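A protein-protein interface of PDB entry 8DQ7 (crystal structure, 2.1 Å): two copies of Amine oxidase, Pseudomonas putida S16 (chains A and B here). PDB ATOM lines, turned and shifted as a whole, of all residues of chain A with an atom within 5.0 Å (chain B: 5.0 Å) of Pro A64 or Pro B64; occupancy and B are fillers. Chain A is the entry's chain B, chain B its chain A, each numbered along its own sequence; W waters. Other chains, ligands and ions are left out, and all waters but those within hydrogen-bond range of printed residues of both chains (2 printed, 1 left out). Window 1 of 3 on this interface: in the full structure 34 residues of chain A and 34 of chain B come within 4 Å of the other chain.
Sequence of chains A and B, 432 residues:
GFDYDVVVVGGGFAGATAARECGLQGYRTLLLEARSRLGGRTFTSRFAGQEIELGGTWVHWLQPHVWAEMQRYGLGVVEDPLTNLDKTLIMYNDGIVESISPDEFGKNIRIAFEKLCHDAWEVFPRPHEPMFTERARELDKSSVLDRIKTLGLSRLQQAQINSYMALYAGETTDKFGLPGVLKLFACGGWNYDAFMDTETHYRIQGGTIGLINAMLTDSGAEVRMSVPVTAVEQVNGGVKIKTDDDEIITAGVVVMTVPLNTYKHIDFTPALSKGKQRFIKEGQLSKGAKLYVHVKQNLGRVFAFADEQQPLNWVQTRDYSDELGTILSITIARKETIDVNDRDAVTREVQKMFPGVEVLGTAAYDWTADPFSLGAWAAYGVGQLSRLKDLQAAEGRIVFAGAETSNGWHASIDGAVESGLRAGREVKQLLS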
ATOM      1  N   TRP A  61      -7.059 -22.550 -16.156  1.00  0.00           N
ATOM      2  CA  TRP A  61      -5.668 -22.479 -15.711  1.00  0.00           C
ATOM      3  C   TRP A  61      -5.536 -21.971 -14.277  1.00  0.00           C
ATOM      4  O   TRP A  61      -4.466 -22.130 -13.683  1.00  0.00           O
ATOM      5  CB  TRP A  61      -4.831 -21.604 -16.651  1.00  0.00           C
ATOM      6  CG  TRP A  61      -5.437 -20.291 -16.945  1.00  0.00           C
ATOM      7  CD1 TRP A  61      -5.301 -19.136 -16.217  1.00  0.00           C
ATOM      8  CD2 TRP A  61      -6.329 -19.980 -18.043  1.00  0.00           C
ATOM      9  NE1 TRP A  61      -6.041 -18.123 -16.794  1.00  0.00           N
ATOM     10  CE2 TRP A  61      -6.668 -18.610 -17.923  1.00  0.00           C
ATOM     11  CE3 TRP A  61      -6.843 -20.726 -19.130  1.00  0.00           C
ATOM     12  CZ2 TRP A  61      -7.508 -17.964 -18.829  1.00  0.00           C
ATOM     13  CZ3 TRP A  61      -7.694 -20.090 -20.032  1.00  0.00           C
ATOM     14  CH2 TRP A  61      -8.021 -18.709 -19.879  1.00  0.00           C
ATOM     15  N   LEU A  62      -6.585 -21.364 -13.708  1.00  0.00           N
ATOM     16  CA  LEU A  62      -6.550 -21.071 -12.285  1.00  0.00           C
ATOM     17  C   LEU A  62      -6.804 -22.307 -11.441  1.00  0.00           C
ATOM     18  O   LEU A  62      -6.744 -22.228 -10.209  1.00  0.00           O
ATOM     19  CB  LEU A  62      -7.570 -19.978 -11.923  1.00  0.00           C
ATOM     20  CG  LEU A  62      -7.298 -18.589 -12.483  1.00  0.00           C
ATOM     21  CD1 LEU A  62      -8.466 -17.620 -12.255  1.00  0.00           C
ATOM     22  CD2 LEU A  62      -5.978 -18.009 -11.925  1.00  0.00           C
ATOM     23  N   GLN A  63      -7.114 -23.455 -12.081  1.00  0.00           N
ATOM     24  CA  GLN A  63      -7.285 -24.702 -11.369  1.00  0.00           C
ATOM     25  C   GLN A  63      -5.954 -25.447 -11.417  1.00  0.00           C
ATOM     26  O   GLN A  63      -5.609 -26.033 -12.451  1.00  0.00           O
ATOM     27  CB  GLN A  63      -8.415 -25.532 -12.005  1.00  0.00           C
ATOM     28  CG  GLN A  63      -9.721 -24.801 -11.862  1.00  0.00           C
ATOM     29  CD  GLN A  63     -10.873 -25.497 -12.535  1.00  0.00           C
ATOM     30  OE1 GLN A  63     -10.683 -26.217 -13.539  1.00  0.00           O
ATOM     31  NE2 GLN A  63     -12.085 -25.286 -12.004  1.00  0.00           N
ATOM     32  N   PRO A  64      -5.168 -25.440 -10.350  1.00  0.00           N
ATOM     33  CA  PRO A  64      -3.744 -25.762 -10.501  1.00  0.00           C
ATOM     34  C   PRO A  64      -3.458 -27.231 -10.831  1.00  0.00           C
ATOM     35  O   PRO A  64      -2.519 -27.501 -11.586  1.00  0.00           O
ATOM     36  CB  PRO A  64      -3.151 -25.354  -9.138  1.00  0.00           C
ATOM     37  CG  PRO A  64      -4.268 -25.459  -8.182  1.00  0.00           C
ATOM     38  CD  PRO A  64      -5.532 -25.099  -8.955  1.00  0.00           C
ATOM     39  N   HIS A  65      -4.236 -28.183 -10.320  1.00  0.00           N
ATOM     40  CA  HIS A  65      -3.865 -29.575 -10.490  1.00  0.00           C
ATOM     41  C   HIS A  65      -4.185 -30.076 -11.895  1.00  0.00           C
ATOM     42  O   HIS A  65      -3.317 -30.688 -12.574  1.00  0.00           O
ATOM     43  CB  HIS A  65      -4.582 -30.414  -9.412  1.00  0.00           C
ATOM     44  CG  HIS A  65      -4.418 -29.851  -8.034  1.00  0.00           C
ATOM     45  ND1 HIS A  65      -5.401 -29.115  -7.409  1.00  0.00           N
ATOM     46  CD2 HIS A  65      -3.374 -29.909  -7.161  1.00  0.00           C
ATOM     47  CE1 HIS A  65      -4.966 -28.737  -6.208  1.00  0.00           C
ATOM     48  NE2 HIS A  65      -3.728 -29.181  -6.054  1.00  0.00           N
ATOM     49  N   VAL A  66      -5.415 -29.814 -12.366  1.00  0.00           N
ATOM     50  CA  VAL A  66      -5.746 -30.235 -13.737  1.00  0.00           C
ATOM     51  C   VAL A  66      -4.894 -29.439 -14.747  1.00  0.00           C
ATOM     52  O   VAL A  66      -4.413 -29.981 -15.757  1.00  0.00           O
ATOM     53  CB  VAL A  66      -7.262 -30.106 -14.001  1.00  0.00           C
ATOM     54  CG1 VAL A  66      -7.743 -28.640 -13.900  1.00  0.00           C
ATOM     55  CG2 VAL A  66      -7.690 -30.702 -15.405  1.00  0.00           C
ATOM     56  N   TRP A  67      -4.655 -28.162 -14.478  1.00  0.00           N
ATOM     57  CA  TRP A  67      -3.818 -27.406 -15.409  1.00  0.00           C
ATOM     58  C   TRP A  67      -2.410 -27.988 -15.481  1.00  0.00           C
ATOM     59  O   TRP A  67      -1.851 -28.111 -16.569  1.00  0.00           O
ATOM     60  CB  TRP A  67      -3.786 -25.932 -15.033  1.00  0.00           C
ATOM     61  CG  TRP A  67      -3.152 -25.118 -16.146  1.00  0.00           C
ATOM     62  CD1 TRP A  67      -1.863 -24.591 -16.188  1.00  0.00           C
ATOM     63  CD2 TRP A  67      -3.767 -24.789 -17.386  1.00  0.00           C
ATOM     64  NE1 TRP A  67      -1.689 -23.933 -17.391  1.00  0.00           N
ATOM     65  CE2 TRP A  67      -2.835 -24.058 -18.141  1.00  0.00           C
ATOM     66  CE3 TRP A  67      -5.030 -25.053 -17.932  1.00  0.00           C
ATOM     67  CZ2 TRP A  67      -3.129 -23.566 -19.424  1.00  0.00           C
ATOM     68  CZ3 TRP A  67      -5.326 -24.571 -19.201  1.00  0.00           C
ATOM     69  CH2 TRP A  67      -4.367 -23.842 -19.939  1.00  0.00           C
ATOM     70  N   ALA A  68      -1.802 -28.354 -14.335  1.00  0.00           N
ATOM     71  CA  ALA A  68      -0.470 -28.927 -14.421  1.00  0.00           C
ATOM     72  C   ALA A  68      -0.495 -30.222 -15.224  1.00  0.00           C
ATOM     73  O   ALA A  68       0.437 -30.506 -15.976  1.00  0.00           O
ATOM     74  CB  ALA A  68       0.120 -29.173 -13.014  1.00  0.00           C
ATOM     75  N   HIS A 128      -7.340 -23.389   0.330  1.00  0.00           N
ATOM     76  CA  HIS A 128      -6.949 -24.800   0.425  1.00  0.00           C
ATOM     77  C   HIS A 128      -6.814 -25.269   1.866  1.00  0.00           C
ATOM     78  O   HIS A 128      -6.434 -26.434   2.084  1.00  0.00           O
ATOM     79  CB  HIS A 128      -5.643 -25.073  -0.356  1.00  0.00           C
ATOM     80  CG  HIS A 128      -5.820 -24.905  -1.835  1.00  0.00           C
ATOM     81  ND1 HIS A 128      -6.256 -25.935  -2.657  1.00  0.00           N
ATOM     82  CD2 HIS A 128      -5.747 -23.800  -2.617  1.00  0.00           C
ATOM     83  CE1 HIS A 128      -6.385 -25.474  -3.892  1.00  0.00           C
ATOM     84  NE2 HIS A 128      -6.101 -24.183  -3.894  1.00  0.00           N
ATOM     85  N   TRP A 409     -10.959 -27.123  -5.255  1.00  0.00           N
ATOM     86  CA  TRP A 409     -12.067 -27.143  -6.233  1.00  0.00           C
ATOM     87  C   TRP A 409     -12.843 -28.456  -6.116  1.00  0.00           C
ATOM     88  O   TRP A 409     -12.773 -29.329  -6.991  1.00  0.00           O
ATOM     89  CB  TRP A 409     -11.511 -26.991  -7.643  1.00  0.00           C
ATOM     90  CG  TRP A 409     -10.867 -25.668  -7.926  1.00  0.00           C
ATOM     91  CD1 TRP A 409      -9.543 -25.329  -7.770  1.00  0.00           C
ATOM     92  CD2 TRP A 409     -11.521 -24.514  -8.429  1.00  0.00           C
ATOM     93  NE1 TRP A 409      -9.341 -24.010  -8.154  1.00  0.00           N
ATOM     94  CE2 TRP A 409     -10.545 -23.487  -8.545  1.00  0.00           C
ATOM     95  CE3 TRP A 409     -12.858 -24.230  -8.775  1.00  0.00           C
ATOM     96  CZ2 TRP A 409     -10.858 -22.222  -9.013  1.00  0.00           C
ATOM     97  CZ3 TRP A 409     -13.165 -22.965  -9.223  1.00  0.00           C
ATOM     98  CH2 TRP A 409     -12.180 -21.982  -9.345  1.00  0.00           C
ATOM     99  N   ASP A 414     -10.681 -30.727 -11.073  1.00  0.00           N
ATOM    100  CA  ASP A 414      -9.459 -30.346 -10.382  1.00  0.00           C
ATOM    101  C   ASP A 414      -9.381 -30.930  -8.974  1.00  0.00           C
ATOM    102  O   ASP A 414      -8.304 -31.388  -8.544  1.00  0.00           O
ATOM    103  CB  ASP A 414      -9.345 -28.824 -10.315  1.00  0.00           C
ATOM    104  CG  ASP A 414      -7.990 -28.402  -9.716  1.00  0.00           C
ATOM    105  OD1 ASP A 414      -7.018 -28.364 -10.478  1.00  0.00           O
ATOM    106  OD2 ASP A 414      -7.939 -28.198  -8.482  1.00  0.00           O
ATOM    107  N   TRP B  61      -1.027 -20.642  -4.450  1.00  0.00           N
ATOM    108  CA  TRP B  61      -1.883 -21.670  -5.024  1.00  0.00           C
ATOM    109  C   TRP B  61      -2.533 -21.223  -6.343  1.00  0.00           C
ATOM    110  O   TRP B  61      -3.056 -22.069  -7.065  1.00  0.00           O
ATOM    111  CB  TRP B  61      -2.958 -22.108  -4.018  1.00  0.00           C
ATOM    112  CG  TRP B  61      -3.713 -20.992  -3.419  1.00  0.00           C
ATOM    113  CD1 TRP B  61      -4.845 -20.393  -3.927  1.00  0.00           C
ATOM    114  CD2 TRP B  61      -3.401 -20.285  -2.196  1.00  0.00           C
ATOM    115  NE1 TRP B  61      -5.255 -19.372  -3.089  1.00  0.00           N
ATOM    116  CE2 TRP B  61      -4.393 -19.287  -2.024  1.00  0.00           C
ATOM    117  CE3 TRP B  61      -2.390 -20.417  -1.227  1.00  0.00           C
ATOM    118  CZ2 TRP B  61      -4.399 -18.414  -0.933  1.00  0.00           C
ATOM    119  CZ3 TRP B  61      -2.395 -19.539  -0.138  1.00  0.00           C
ATOM    120  CH2 TRP B  61      -3.394 -18.552   0.001  1.00  0.00           C
ATOM    121  N   LEU B  62      -2.530 -19.933  -6.669  1.00  0.00           N
ATOM    122  CA  LEU B  62      -2.945 -19.551  -8.009  1.00  0.00           C
ATOM    123  C   LEU B  62      -1.861 -19.812  -9.039  1.00  0.00           C
ATOM    124  O   LEU B  62      -2.095 -19.597 -10.234  1.00  0.00           O
ATOM    125  CB  LEU B  62      -3.347 -18.078  -8.075  1.00  0.00           C
ATOM    126  CG  LEU B  62      -4.606 -17.718  -7.297  1.00  0.00           C
ATOM    127  CD1 LEU B  62      -4.811 -16.197  -7.246  1.00  0.00           C
ATOM    128  CD2 LEU B  62      -5.849 -18.419  -7.877  1.00  0.00           C
ATOM    129  N   GLN B  63      -0.668 -20.258  -8.597  1.00  0.00           N
ATOM    130  CA  GLN B  63       0.390 -20.616  -9.522  1.00  0.00           C
ATOM    131  C   GLN B  63       0.317 -22.123  -9.742  1.00  0.00           C
ATOM    132  O   GLN B  63       0.720 -22.904  -8.864  1.00  0.00           O
ATOM    133  CB  GLN B  63       1.758 -20.196  -8.971  1.00  0.00           C
ATOM    134  CG  GLN B  63       1.805 -18.732  -8.806  1.00  0.00           C
ATOM    135  CD  GLN B  63       3.070 -18.247  -8.134  1.00  0.00           C
ATOM    136  OE1 GLN B  63       3.664 -18.962  -7.305  1.00  0.00           O
ATOM    137  NE2 GLN B  63       3.490 -17.022  -8.489  1.00  0.00           N
ATOM    138  N   PRO B  64      -0.187 -22.580 -10.888  1.00  0.00           N
ATOM    139  CA  PRO B  64      -0.637 -23.974 -10.975  1.00  0.00           C
ATOM    140  C   PRO B  64       0.492 -25.002 -10.912  1.00  0.00           C
ATOM    141  O   PRO B  64       0.318 -26.056 -10.293  1.00  0.00           O
ATOM    142  CB  PRO B  64      -1.378 -24.008 -12.325  1.00  0.00           C
ATOM    143  CG  PRO B  64      -0.801 -22.860 -13.113  1.00  0.00           C
ATOM    144  CD  PRO B  64      -0.476 -21.797 -12.106  1.00  0.00           C
ATOM    145  N   HIS B  65       1.644 -24.741 -11.536  1.00  0.00           N
ATOM    146  CA  HIS B  65       2.644 -25.791 -11.639  1.00  0.00           C
ATOM    147  C   HIS B  65       3.379 -26.017 -10.318  1.00  0.00           C
ATOM    148  O   HIS B  65       3.496 -27.175  -9.829  1.00  0.00           O
ATOM    149  CB  HIS B  65       3.615 -25.429 -12.785  1.00  0.00           C
ATOM    150  CG  HIS B  65       2.899 -25.002 -14.033  1.00  0.00           C
ATOM    151  ND1 HIS B  65       2.702 -23.679 -14.366  1.00  0.00           N
ATOM    152  CD2 HIS B  65       2.309 -25.731 -15.022  1.00  0.00           C
ATOM    153  CE1 HIS B  65       2.034 -23.608 -15.516  1.00  0.00           C
ATOM    154  NE2 HIS B  65       1.767 -24.841 -15.915  1.00  0.00           N
ATOM    155  N   VAL B  66       3.835 -24.933  -9.687  1.00  0.00           N
ATOM    156  CA  VAL B  66       4.509 -25.125  -8.396  1.00  0.00           C
ATOM    157  C   VAL B  66       3.509 -25.639  -7.348  1.00  0.00           C
ATOM    158  O   VAL B  66       3.840 -26.477  -6.487  1.00  0.00           O
ATOM    159  CB  VAL B  66       5.222 -23.831  -7.945  1.00  0.00           C
ATOM    160  CG1 VAL B  66       4.212 -22.681  -7.679  1.00  0.00           C
ATOM    161  CG2 VAL B  66       6.068 -24.083  -6.650  1.00  0.00           C
ATOM    162  N   TRP B  67       2.273 -25.151  -7.393  1.00  0.00           N
ATOM    163  CA  TRP B  67       1.302 -25.644  -6.408  1.00  0.00           C
ATOM    164  C   TRP B  67       1.052 -27.138  -6.595  1.00  0.00           C
ATOM    165  O   TRP B  67       1.011 -27.888  -5.622  1.00  0.00           O
ATOM    166  CB  TRP B  67      -0.009 -24.862  -6.492  1.00  0.00           C
ATOM    167  CG  TRP B  67      -0.907 -25.210  -5.320  1.00  0.00           C
ATOM    168  CD1 TRP B  67      -1.992 -26.059  -5.321  1.00  0.00           C
ATOM    169  CD2 TRP B  67      -0.756 -24.742  -3.985  1.00  0.00           C
ATOM    170  NE1 TRP B  67      -2.514 -26.139  -4.041  1.00  0.00           N
ATOM    171  CE2 TRP B  67      -1.766 -25.340  -3.211  1.00  0.00           C
ATOM    172  CE3 TRP B  67       0.176 -23.893  -3.356  1.00  0.00           C
ATOM    173  CZ2 TRP B  67      -1.908 -25.085  -1.839  1.00  0.00           C
ATOM    174  CZ3 TRP B  67       0.033 -23.639  -1.990  1.00  0.00           C
ATOM    175  CH2 TRP B  67      -1.001 -24.243  -1.253  1.00  0.00           C
ATOM    176  N   ALA B  68       0.880 -27.604  -7.842  1.00  0.00           N
ATOM    177  CA  ALA B  68       0.689 -29.041  -8.012  1.00  0.00           C
ATOM    178  C   ALA B  68       1.877 -29.817  -7.451  1.00  0.00           C
ATOM    179  O   ALA B  68       1.695 -30.878  -6.836  1.00  0.00           O
ATOM    180  CB  ALA B  68       0.479 -29.385  -9.492  1.00  0.00           C
ATOM    181  N   HIS B 128      -1.840 -17.736 -20.709  1.00  0.00           N
ATOM    182  CA  HIS B 128      -0.865 -18.758 -21.104  1.00  0.00           C
ATOM    183  C   HIS B 128      -0.686 -18.850 -22.612  1.00  0.00           C
ATOM    184  O   HIS B 128       0.044 -19.740 -23.079  1.00  0.00           O
ATOM    185  CB  HIS B 128      -1.257 -20.151 -20.548  1.00  0.00           C
ATOM    186  CG  HIS B 128      -1.153 -20.213 -19.062  1.00  0.00           C
ATOM    187  ND1 HIS B 128       0.031 -20.522 -18.413  1.00  0.00           N
ATOM    188  CD2 HIS B 128      -2.046 -19.889 -18.099  1.00  0.00           C
ATOM    189  CE1 HIS B 128      -0.170 -20.445 -17.108  1.00  0.00           C
ATOM    190  NE2 HIS B 128      -1.412 -20.045 -16.894  1.00  0.00           N
ATOM    191  N   TRP B 409       3.764 -17.616 -15.578  1.00  0.00           N
ATOM    192  CA  TRP B 409       4.439 -16.878 -14.494  1.00  0.00           C
ATOM    193  C   TRP B 409       5.950 -16.817 -14.757  1.00  0.00           C
ATOM    194  O   TRP B 409       6.763 -17.436 -14.057  1.00  0.00           O
ATOM    195  CB  TRP B 409       4.153 -17.555 -13.162  1.00  0.00           C
ATOM    196  CG  TRP B 409       2.738 -17.451 -12.697  1.00  0.00           C
ATOM    197  CD1 TRP B 409       1.719 -18.362 -12.895  1.00  0.00           C
ATOM    198  CD2 TRP B 409       2.174 -16.385 -11.936  1.00  0.00           C
ATOM    199  NE1 TRP B 409       0.551 -17.917 -12.283  1.00  0.00           N
ATOM    200  CE2 TRP B 409       0.805 -16.700 -11.704  1.00  0.00           C
ATOM    201  CE3 TRP B 409       2.688 -15.174 -11.434  1.00  0.00           C
ATOM    202  CZ2 TRP B 409      -0.037 -15.854 -10.989  1.00  0.00           C
ATOM    203  CZ3 TRP B 409       1.844 -14.340 -10.732  1.00  0.00           C
ATOM    204  CH2 TRP B 409       0.501 -14.682 -10.510  1.00  0.00           C
ATOM    205  N   ASP B 414       7.263 -20.729 -10.579  1.00  0.00           N
ATOM    206  CA  ASP B 414       6.215 -21.445 -11.299  1.00  0.00           C
ATOM    207  C   ASP B 414       6.520 -21.551 -12.781  1.00  0.00           C
ATOM    208  O   ASP B 414       6.306 -22.614 -13.387  1.00  0.00           O
ATOM    209  CB  ASP B 414       4.865 -20.745 -11.111  1.00  0.00           C
ATOM    210  CG  ASP B 414       3.729 -21.556 -11.744  1.00  0.00           C
ATOM    211  OD1 ASP B 414       3.243 -22.476 -11.065  1.00  0.00           O
ATOM    212  OD2 ASP B 414       3.384 -21.285 -12.902  1.00  0.00           O
HETATM  213  O   HOH W   1      -2.484 -20.340 -14.439  1.00  0.00           O
HETATM  214  O   HOH W   2      -5.434 -22.973  -6.191  1.00  0.00           O
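The backbone carbonyl oxygen of Pro A64 lies close to the backbone carbonyl oxygen of Pro B64, 3.4 Å away.
Water W2 lies within hydrogen-bond range of a ring nitrogen (NE2) of His A128 (2.7 Å) and the backbone carbonyl oxygen (O) of Trp B61 (2.7 Å).
Water W1 lies within hydrogen-bond range of NE2 of His B128 (2.7 Å) and O of Trp A61 (2.8 Å).
Of the printed residues of chain B, Trp A61 touches Pro B64 and His B128.
Of chain B, only Trp B61 (3.8 Å), Pro B64 (3.4 Å) and Trp B67 (3.7 Å) come within 4 Å of Pro A64.
Printed residues of chain B within 4 Å of His A65: Trp B67.
Leu B62 touches none of the printed residues of chain A.
Printed residues of chain A within 4 Å of Pro B64: Trp A61 (3.8 Å), Pro A64 (3.4 Å) and Trp A67 (3.7 Å).
Of the printed residues of chain A, His B128 touches Trp A61 (3.6 Å) and Trp A67 (3.8 Å).
The nearest residue of chain A that does not touch Pro B64 is Ala A68 (4.1 Å).
The nearest printed residue of chain B that does not touch Trp A61 is Leu B62 (4.9 Å).
Pro A64 touches its own counterpart, Pro B64.
Pro A64 touches Trp B67, and with the chains exchanged Trp A67 touches Pro B64.
His A65 touches Trp B67, and with the chains exchanged Trp A67 touches His B65.
Trp A67 touches His B128, and with the chains exchanged His A128 touches Trp B67.
Among the printed residues, merely in contact across the chains: Ala A68 with Ala B68 (3.5 Å), His A128 with Trp B61 (3.6 Å), Trp A61 with His B128 (3.6 Å), His A65 with Trp B67 (3.6 Å), Trp A67 with His B65 (3.6 Å), Trp A67 with Pro B64 (3.7 Å), Pro A64 with Trp B67 (3.7 Å), Pro A64 with Trp B61 (3.8 Å), Trp A61 with Pro B64 (3.8 Å), Trp A67 with His B128 (3.8 Å) and His A128 with Trp B67 (3.9 Å).
Of the 11 printed residues of chain A, 6 touch a printed residue of chain B.
Hydrophobic or aromatic side chains of chain A that line the printed part of chain B: Trp A61, Pro A64, His A65, Trp A67, Ala A68 and His A128.
Along chain A the printed residues that touch a printed residue of chain B span positions 61 to 128.
Of the 11 printed residues of chain B, 6 touch a printed residue of chain A.
Hydrophobic or aromatic side chains of chain B that line the printed part of chain A: Trp B61, Pro B64, His B65, Trp B67, Ala B68 and His B128.
N of His B65 lies within hydrogen-bond range of OD1 of Asp B414, at 2.8 Å.
N of His A65 sits at hydrogen-bond distance from OD1 of Asp A414, 2.8 Å away.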
